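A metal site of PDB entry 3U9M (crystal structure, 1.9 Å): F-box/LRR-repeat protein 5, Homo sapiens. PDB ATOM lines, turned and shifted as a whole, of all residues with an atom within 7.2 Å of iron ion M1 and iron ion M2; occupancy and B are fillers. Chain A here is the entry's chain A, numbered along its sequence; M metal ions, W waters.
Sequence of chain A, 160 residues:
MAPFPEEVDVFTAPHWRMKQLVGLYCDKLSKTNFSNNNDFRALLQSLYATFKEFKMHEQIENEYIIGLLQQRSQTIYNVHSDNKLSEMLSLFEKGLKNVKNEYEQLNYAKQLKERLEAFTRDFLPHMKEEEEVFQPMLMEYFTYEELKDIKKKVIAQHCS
Iron ion M1 is bound by water W1 (2.1 Å), the side-chain carboxylate (OE2) of Glu 61 (2.1 Å), the side-chain carboxylate (OE1) of Glu 130 (2.2 Å), a ring nitrogen (NE2) of His 15 (2.2 Å) and a ring nitrogen (NE2) of His 57 (2.3 Å).
Iron ion M1 has five donor atoms within binding distance.
Iron ion M2 is bound by the side-chain carboxylate of Glu 130 (2.0 Å), a ring nitrogen (NE2) of His 80 (2.2 Å), water W1 (2.2 Å), the side-chain carboxylate of Glu 58 (2.2 Å), the side-chain carboxylate of Glu 61 (2.2 Å) and a ring nitrogen (NE2) of His 126 (2.3 Å).
Iron ion M2 has six donor atoms within binding distance.
Five residues have an atom within 4 Å of iron ion M2: Glu 58, Glu 61, His 80, His 126 and Glu 130.
The backbone carbonyl oxygen (O) of Glu 61 is in hydrogen-bond range of the backbone NH (N) of Ile 66 (2.8 Å).
ND1 of His 126 lies within hydrogen-bond range of OG of Ser 81 (2.6 Å).
O of Glu 58 sits close to ND2 of Asn 62 (3.5 Å).
The side-chain amide oxygen of Asn 83 lies within hydrogen-bond range of a ring nitrogen (ND1) of His 126, 3.3 Å away.
OE2 of Glu 131 lies within hydrogen-bond range of ND1 of His 15, 2.4 Å away.
ND1 of His 15 lies close to O of Phe 11 (3.3 Å).
ND1 of His 57 sits at hydrogen-bond distance from NE2 of His 158.
A ring nitrogen (ND1) of His 80 lies within hydrogen-bond range of the side-chain amide oxygen of Asn 62 (2.5 Å).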
ATOM      1  N   VAL A  10      26.628  10.835  24.868  1.00  0.00           N
ATOM      2  CA  VAL A  10      25.788  11.834  25.528  1.00  0.00           C
ATOM      3  C   VAL A  10      25.318  12.972  24.613  1.00  0.00           C
ATOM      4  O   VAL A  10      24.658  13.894  25.092  1.00  0.00           O
ATOM      5  CB  VAL A  10      26.488  12.447  26.749  1.00  0.00           C
ATOM      6  CG1 VAL A  10      26.877  11.360  27.742  1.00  0.00           C
ATOM      7  CG2 VAL A  10      27.696  13.288  26.320  1.00  0.00           C
ATOM      8  N   PHE A  11      25.649  12.897  23.333  1.00  0.00           N
ATOM      9  CA  PHE A  11      25.397  14.023  22.414  1.00  0.00           C
ATOM     10  C   PHE A  11      24.550  13.686  21.181  1.00  0.00           C
ATOM     11  O   PHE A  11      23.764  14.511  20.721  1.00  0.00           O
ATOM     12  CB  PHE A  11      26.728  14.635  21.947  1.00  0.00           C
ATOM     13  CG  PHE A  11      27.492  15.339  23.020  1.00  0.00           C
ATOM     14  CD1 PHE A  11      26.948  16.445  23.682  1.00  0.00           C
ATOM     15  CD2 PHE A  11      28.766  14.926  23.368  1.00  0.00           C
ATOM     16  CE1 PHE A  11      27.660  17.101  24.672  1.00  0.00           C
ATOM     17  CE2 PHE A  11      29.488  15.572  24.359  1.00  0.00           C
ATOM     18  CZ  PHE A  11      28.924  16.669  25.015  1.00  0.00           C
ATOM     19  N   PRO A  14      20.291  13.629  21.542  1.00  0.00           N
ATOM     20  CA  PRO A  14      19.836  15.003  21.732  1.00  0.00           C
ATOM     21  C   PRO A  14      20.064  15.855  20.479  1.00  0.00           C
ATOM     22  O   PRO A  14      19.154  16.583  20.077  1.00  0.00           O
ATOM     23  CB  PRO A  14      20.727  15.503  22.875  1.00  0.00           C
ATOM     24  CG  PRO A  14      20.974  14.273  23.674  1.00  0.00           C
ATOM     25  CD  PRO A  14      21.123  13.172  22.672  1.00  0.00           C
ATOM     26  N   HIS A  15      21.244  15.749  19.891  1.00  0.00           N
ATOM     27  CA  HIS A  15      21.551  16.495  18.667  1.00  0.00           C
ATOM     28  C   HIS A  15      20.669  16.113  17.479  1.00  0.00           C
ATOM     29  O   HIS A  15      20.413  16.931  16.590  1.00  0.00           O
ATOM     30  CB  HIS A  15      23.031  16.343  18.302  1.00  0.00           C
ATOM     31  CG  HIS A  15      23.955  17.088  19.216  1.00  0.00           C
ATOM     32  ND1 HIS A  15      25.331  16.978  19.131  1.00  0.00           N
ATOM     33  CD2 HIS A  15      23.717  17.946  20.232  1.00  0.00           C
ATOM     34  CE1 HIS A  15      25.891  17.737  20.051  1.00  0.00           C
ATOM     35  NE2 HIS A  15      24.930  18.341  20.738  1.00  0.00           N
ATOM     36  N   MET A  18      17.874  18.301  18.087  1.00  0.00           N
ATOM     37  CA  MET A  18      18.264  19.680  17.800  1.00  0.00           C
ATOM     38  C   MET A  18      18.319  19.943  16.302  1.00  0.00           C
ATOM     39  O   MET A  18      17.799  20.950  15.816  1.00  0.00           O
ATOM     40  CB  MET A  18      19.606  20.028  18.471  1.00  0.00           C
ATOM     41  CG  MET A  18      19.591  19.891  19.997  1.00  0.00           C
ATOM     42  SD  MET A  18      18.190  20.710  20.780  1.00  0.00           S
ATOM     43  CE  MET A  18      17.392  19.315  21.580  1.00  0.00           C
ATOM     44  N   PHE A  54      16.248  24.718  22.703  1.00  0.00           N
ATOM     45  CA  PHE A  54      17.706  24.790  22.541  1.00  0.00           C
ATOM     46  C   PHE A  54      18.346  25.187  23.862  1.00  0.00           C
ATOM     47  O   PHE A  54      19.336  24.594  24.305  1.00  0.00           O
ATOM     48  CB  PHE A  54      18.089  25.824  21.482  1.00  0.00           C
ATOM     49  CG  PHE A  54      17.826  25.394  20.062  1.00  0.00           C
ATOM     50  CD1 PHE A  54      17.574  24.071  19.735  1.00  0.00           C
ATOM     51  CD2 PHE A  54      17.842  26.329  19.034  1.00  0.00           C
ATOM     52  CE1 PHE A  54      17.327  23.697  18.422  1.00  0.00           C
ATOM     53  CE2 PHE A  54      17.608  25.965  17.715  1.00  0.00           C
ATOM     54  CZ  PHE A  54      17.350  24.649  17.409  1.00  0.00           C
ATOM     55  N   HIS A  57      18.348  22.440  26.193  1.00  0.00           N
ATOM     56  CA  HIS A  57      19.383  21.493  25.783  1.00  0.00           C
ATOM     57  C   HIS A  57      20.758  21.892  26.303  1.00  0.00           C
ATOM     58  O   HIS A  57      21.486  21.054  26.860  1.00  0.00           O
ATOM     59  CB  HIS A  57      19.423  21.336  24.255  1.00  0.00           C
ATOM     60  CG  HIS A  57      20.604  20.570  23.764  1.00  0.00           C
ATOM     61  ND1 HIS A  57      20.722  19.205  23.900  1.00  0.00           N
ATOM     62  CD2 HIS A  57      21.740  20.977  23.130  1.00  0.00           C
ATOM     63  CE1 HIS A  57      21.858  18.799  23.374  1.00  0.00           C
ATOM     64  NE2 HIS A  57      22.498  19.856  22.902  1.00  0.00           N
ATOM     65  N   GLU A  58      21.121  23.154  26.129  1.00  0.00           N
ATOM     66  CA  GLU A  58      22.411  23.654  26.597  1.00  0.00           C
ATOM     67  C   GLU A  58      22.508  23.588  28.112  1.00  0.00           C
ATOM     68  O   GLU A  58      23.553  23.240  28.667  1.00  0.00           O
ATOM     69  CB  GLU A  58      22.678  25.101  26.128  1.00  0.00           C
ATOM     70  CG  GLU A  58      22.560  25.310  24.607  1.00  0.00           C
ATOM     71  CD  GLU A  58      23.531  24.446  23.835  1.00  0.00           C
ATOM     72  OE1 GLU A  58      24.532  24.004  24.417  1.00  0.00           O
ATOM     73  OE2 GLU A  58      23.279  24.196  22.641  1.00  0.00           O
ATOM     74  N   GLN A  59      21.408  23.901  28.793  1.00  0.00           N
ATOM     75  CA  GLN A  59      21.384  23.834  30.253  1.00  0.00           C
ATOM     76  C   GLN A  59      21.602  22.422  30.777  1.00  0.00           C
ATOM     77  O   GLN A  59      22.375  22.206  31.715  1.00  0.00           O
ATOM     78  CB  GLN A  59      20.070  24.400  30.816  1.00  0.00           C
ATOM     79  CG  GLN A  59      19.999  24.365  32.340  1.00  0.00           C
ATOM     80  CD  GLN A  59      18.743  25.012  32.899  1.00  0.00           C
ATOM     81  OE1 GLN A  59      18.101  25.822  32.247  1.00  0.00           O
ATOM     82  NE2 GLN A  59      18.390  24.639  34.131  1.00  0.00           N
ATOM     83  N   GLU A  61      23.236  20.040  29.319  1.00  0.00           N
ATOM     84  CA  GLU A  61      24.668  19.795  29.116  1.00  0.00           C
ATOM     85  C   GLU A  61      25.536  20.468  30.183  1.00  0.00           C
ATOM     86  O   GLU A  61      26.436  19.832  30.721  1.00  0.00           O
ATOM     87  CB  GLU A  61      25.097  20.239  27.726  1.00  0.00           C
ATOM     88  CG  GLU A  61      24.507  19.385  26.628  1.00  0.00           C
ATOM     89  CD  GLU A  61      24.853  19.899  25.256  1.00  0.00           C
ATOM     90  OE1 GLU A  61      25.012  21.130  25.104  1.00  0.00           O
ATOM     91  OE2 GLU A  61      24.986  19.069  24.330  1.00  0.00           O
ATOM     92  N   ASN A  62      25.274  21.732  30.484  1.00  0.00           N
ATOM     93  CA  ASN A  62      26.003  22.429  31.537  1.00  0.00           C
ATOM     94  C   ASN A  62      25.856  21.750  32.909  1.00  0.00           C
ATOM     95  O   ASN A  62      26.832  21.591  33.639  1.00  0.00           O
ATOM     96  CB  ASN A  62      25.584  23.909  31.615  1.00  0.00           C
ATOM     97  CG  ASN A  62      26.134  24.741  30.470  1.00  0.00           C
ATOM     98  OD1 ASN A  62      27.184  24.443  29.903  1.00  0.00           O
ATOM     99  ND2 ASN A  62      25.423  25.811  30.128  1.00  0.00           N
ATOM    100  N   ILE A  66      29.091  19.126  31.348  1.00  0.00           N
ATOM    101  CA  ILE A  66      30.255  20.011  31.322  1.00  0.00           C
ATOM    102  C   ILE A  66      30.819  20.289  32.710  1.00  0.00           C
ATOM    103  O   ILE A  66      32.033  20.274  32.898  1.00  0.00           O
ATOM    104  CB  ILE A  66      29.935  21.358  30.624  1.00  0.00           C
ATOM    105  CG1 ILE A  66      29.272  21.108  29.265  1.00  0.00           C
ATOM    106  CG2 ILE A  66      31.200  22.197  30.484  1.00  0.00           C
ATOM    107  CD1 ILE A  66      30.054  20.173  28.368  1.00  0.00           C
ATOM    108  N   HIS A  80      32.224  25.330  27.119  1.00  0.00           N
ATOM    109  CA  HIS A  80      30.966  25.059  26.461  1.00  0.00           C
ATOM    110  C   HIS A  80      30.387  26.403  26.026  1.00  0.00           C
ATOM    111  O   HIS A  80      29.894  27.161  26.853  1.00  0.00           O
ATOM    112  CB  HIS A  80      30.011  24.324  27.393  1.00  0.00           C
ATOM    113  CG  HIS A  80      28.703  23.971  26.751  1.00  0.00           C
ATOM    114  ND1 HIS A  80      27.523  23.927  27.465  1.00  0.00           N
ATOM    115  CD2 HIS A  80      28.395  23.632  25.478  1.00  0.00           C
ATOM    116  CE1 HIS A  80      26.544  23.594  26.645  1.00  0.00           C
ATOM    117  NE2 HIS A  80      27.045  23.406  25.439  1.00  0.00           N
ATOM    118  N   SER A  81      30.463  26.688  24.726  1.00  0.00           N
ATOM    119  CA  SER A  81      30.099  28.008  24.222  1.00  0.00           C
ATOM    120  C   SER A  81      28.630  28.339  24.468  1.00  0.00           C
ATOM    121  O   SER A  81      27.815  27.454  24.737  1.00  0.00           O
ATOM    122  CB  SER A  81      30.426  28.146  22.730  1.00  0.00           C
ATOM    123  OG  SER A  81      29.380  27.640  21.930  1.00  0.00           O
ATOM    124  N   ASP A  82      28.294  29.623  24.354  1.00  0.00           N
ATOM    125  CA  ASP A  82      26.959  30.114  24.670  1.00  0.00           C
ATOM    126  C   ASP A  82      25.967  29.867  23.534  1.00  0.00           C
ATOM    127  O   ASP A  82      24.842  29.406  23.765  1.00  0.00           O
ATOM    128  CB  ASP A  82      27.036  31.612  24.993  1.00  0.00           C
ATOM    129  CG  ASP A  82      25.732  32.173  25.516  1.00  0.00           C
ATOM    130  OD1 ASP A  82      24.682  31.904  24.895  1.00  0.00           O
ATOM    131  OD2 ASP A  82      25.753  32.875  26.540  1.00  0.00           O
ATOM    132  N   ASN A  83      26.376  30.177  22.308  1.00  0.00           N
ATOM    133  CA  ASN A  83      25.497  30.165  21.142  1.00  0.00           C
ATOM    134  C   ASN A  83      24.529  31.354  21.122  1.00  0.00           C
ATOM    135  O   ASN A  83      23.713  31.487  20.213  1.00  0.00           O
ATOM    136  CB  ASN A  83      24.748  28.843  21.002  1.00  0.00           C
ATOM    137  CG  ASN A  83      25.624  27.716  20.450  1.00  0.00           C
ATOM    138  OD1 ASN A  83      26.712  27.966  19.928  1.00  0.00           O
ATOM    139  ND2 ASN A  83      25.153  26.484  20.568  1.00  0.00           N
ATOM    140  N   PHE A 123      25.799  27.197  15.506  1.00  0.00           N
ATOM    141  CA  PHE A 123      25.225  26.064  16.216  1.00  0.00           C
ATOM    142  C   PHE A 123      25.728  24.716  15.698  1.00  0.00           C
ATOM    143  O   PHE A 123      25.997  23.821  16.485  1.00  0.00           O
ATOM    144  CB  PHE A 123      23.689  26.126  16.155  1.00  0.00           C
ATOM    145  CG  PHE A 123      22.995  25.137  17.072  1.00  0.00           C
ATOM    146  CD1 PHE A 123      23.627  24.623  18.201  1.00  0.00           C
ATOM    147  CD2 PHE A 123      21.695  24.739  16.813  1.00  0.00           C
ATOM    148  CE1 PHE A 123      22.983  23.736  19.031  1.00  0.00           C
ATOM    149  CE2 PHE A 123      21.048  23.831  17.649  1.00  0.00           C
ATOM    150  CZ  PHE A 123      21.688  23.341  18.753  1.00  0.00           C
ATOM    151  N   HIS A 126      29.222  23.933  16.777  1.00  0.00           N
ATOM    152  CA  HIS A 126      29.134  23.787  18.229  1.00  0.00           C
ATOM    153  C   HIS A 126      28.796  22.343  18.616  1.00  0.00           C
ATOM    154  O   HIS A 126      29.489  21.722  19.423  1.00  0.00           O
ATOM    155  CB  HIS A 126      28.043  24.717  18.768  1.00  0.00           C
ATOM    156  CG  HIS A 126      27.787  24.563  20.225  1.00  0.00           C
ATOM    157  ND1 HIS A 126      28.346  25.410  21.167  1.00  0.00           N
ATOM    158  CD2 HIS A 126      27.043  23.677  20.922  1.00  0.00           C
ATOM    159  CE1 HIS A 126      27.948  25.041  22.377  1.00  0.00           C
ATOM    160  NE2 HIS A 126      27.148  23.991  22.251  1.00  0.00           N
ATOM    161  N   MET A 127      27.719  21.834  18.048  1.00  0.00           N
ATOM    162  CA  MET A 127      27.311  20.463  18.289  1.00  0.00           C
ATOM    163  C   MET A 127      28.408  19.495  17.873  1.00  0.00           C
ATOM    164  O   MET A 127      28.743  18.568  18.601  1.00  0.00           O
ATOM    165  CB  MET A 127      26.019  20.177  17.525  1.00  0.00           C
ATOM    166  CG  MET A 127      24.797  20.834  18.147  1.00  0.00           C
ATOM    167  SD  MET A 127      23.247  20.218  17.464  1.00  0.00           S
ATOM    168  CE  MET A 127      23.270  20.995  15.841  1.00  0.00           C
ATOM    169  N   LYS A 128      28.968  19.726  16.688  1.00  0.00           N
ATOM    170  CA  LYS A 128      30.012  18.869  16.147  1.00  0.00           C
ATOM    171  C   LYS A 128      31.219  18.798  17.079  1.00  0.00           C
ATOM    172  O   LYS A 128      31.808  17.733  17.261  1.00  0.00           O
ATOM    173  CB  LYS A 128      30.433  19.373  14.763  1.00  0.00           C
ATOM    174  CG  LYS A 128      31.438  18.490  14.050  1.00  0.00           C
ATOM    175  CD  LYS A 128      31.957  19.185  12.804  1.00  0.00           C
ATOM    176  CE  LYS A 128      33.110  18.409  12.178  1.00  0.00           C
ATOM    177  NZ  LYS A 128      33.811  19.220  11.165  1.00  0.00           N
ATOM    178  N   GLU A 130      31.218  19.155  20.310  1.00  0.00           N
ATOM    179  CA  GLU A 130      30.849  18.313  21.431  1.00  0.00           C
ATOM    180  C   GLU A 130      31.053  16.846  21.075  1.00  0.00           C
ATOM    181  O   GLU A 130      31.633  16.089  21.853  1.00  0.00           O
ATOM    182  CB  GLU A 130      29.414  18.589  21.847  1.00  0.00           C
ATOM    183  CG  GLU A 130      29.248  19.933  22.500  1.00  0.00           C
ATOM    184  CD  GLU A 130      27.811  20.329  22.639  1.00  0.00           C
ATOM    185  OE1 GLU A 130      26.943  19.730  21.970  1.00  0.00           O
ATOM    186  OE2 GLU A 130      27.542  21.240  23.434  1.00  0.00           O
ATOM    187  N   GLU A 131      30.605  16.466  19.893  1.00  0.00           N
ATOM    188  CA  GLU A 131      30.688  15.071  19.461  1.00  0.00           C
ATOM    189  C   GLU A 131      32.120  14.635  19.180  1.00  0.00           C
ATOM    190  O   GLU A 131      32.482  13.499  19.457  1.00  0.00           O
ATOM    191  CB  GLU A 131      29.841  14.858  18.213  1.00  0.00           C
ATOM    192  CG  GLU A 131      28.342  15.008  18.457  1.00  0.00           C
ATOM    193  CD  GLU A 131      27.592  15.322  17.183  1.00  0.00           C
ATOM    194  OE1 GLU A 131      28.109  15.006  16.089  1.00  0.00           O
ATOM    195  OE2 GLU A 131      26.492  15.904  17.263  1.00  0.00           O
ATOM    196  N   PHE A 134      34.535  16.816  22.967  1.00  0.00           N
ATOM    197  CA  PHE A 134      34.099  16.556  24.339  1.00  0.00           C
ATOM    198  C   PHE A 134      33.867  15.072  24.634  1.00  0.00           C
ATOM    199  O   PHE A 134      34.271  14.591  25.695  1.00  0.00           O
ATOM    200  CB  PHE A 134      32.867  17.383  24.688  1.00  0.00           C
ATOM    201  CG  PHE A 134      33.139  18.861  24.780  1.00  0.00           C
ATOM    202  CD1 PHE A 134      34.308  19.328  25.346  1.00  0.00           C
ATOM    203  CD2 PHE A 134      32.222  19.774  24.286  1.00  0.00           C
ATOM    204  CE1 PHE A 134      34.569  20.688  25.419  1.00  0.00           C
ATOM    205  CE2 PHE A 134      32.471  21.143  24.367  1.00  0.00           C
ATOM    206  CZ  PHE A 134      33.639  21.590  24.930  1.00  0.00           C
ATOM    207  N   HIS A 158      16.011  15.102  28.517  1.00  0.00           N
ATOM    208  CA  HIS A 158      15.538  15.490  27.194  1.00  0.00           C
ATOM    209  C   HIS A 158      14.152  14.909  26.950  1.00  0.00           C
ATOM    210  O   HIS A 158      13.365  15.491  26.215  1.00  0.00           O
ATOM    211  CB  HIS A 158      16.523  15.054  26.108  1.00  0.00           C
ATOM    212  CG  HIS A 158      17.697  15.965  25.974  1.00  0.00           C
ATOM    213  ND1 HIS A 158      18.812  15.873  26.783  1.00  0.00           N
ATOM    214  CD2 HIS A 158      17.927  17.001  25.134  1.00  0.00           C
ATOM    215  CE1 HIS A 158      19.680  16.807  26.441  1.00  0.00           C
ATOM    216  NE2 HIS A 158      19.167  17.503  25.443  1.00  0.00           N
HETATM  217 FE    FE M   1      24.761  19.869  22.358  1.00  0.00          FE
HETATM  218 FE    FE M   2      26.025  22.557  23.709  1.00  0.00          FE
HETATM  219  O   HOH W   1      24.914  21.938  21.934  1.00  0.00           O
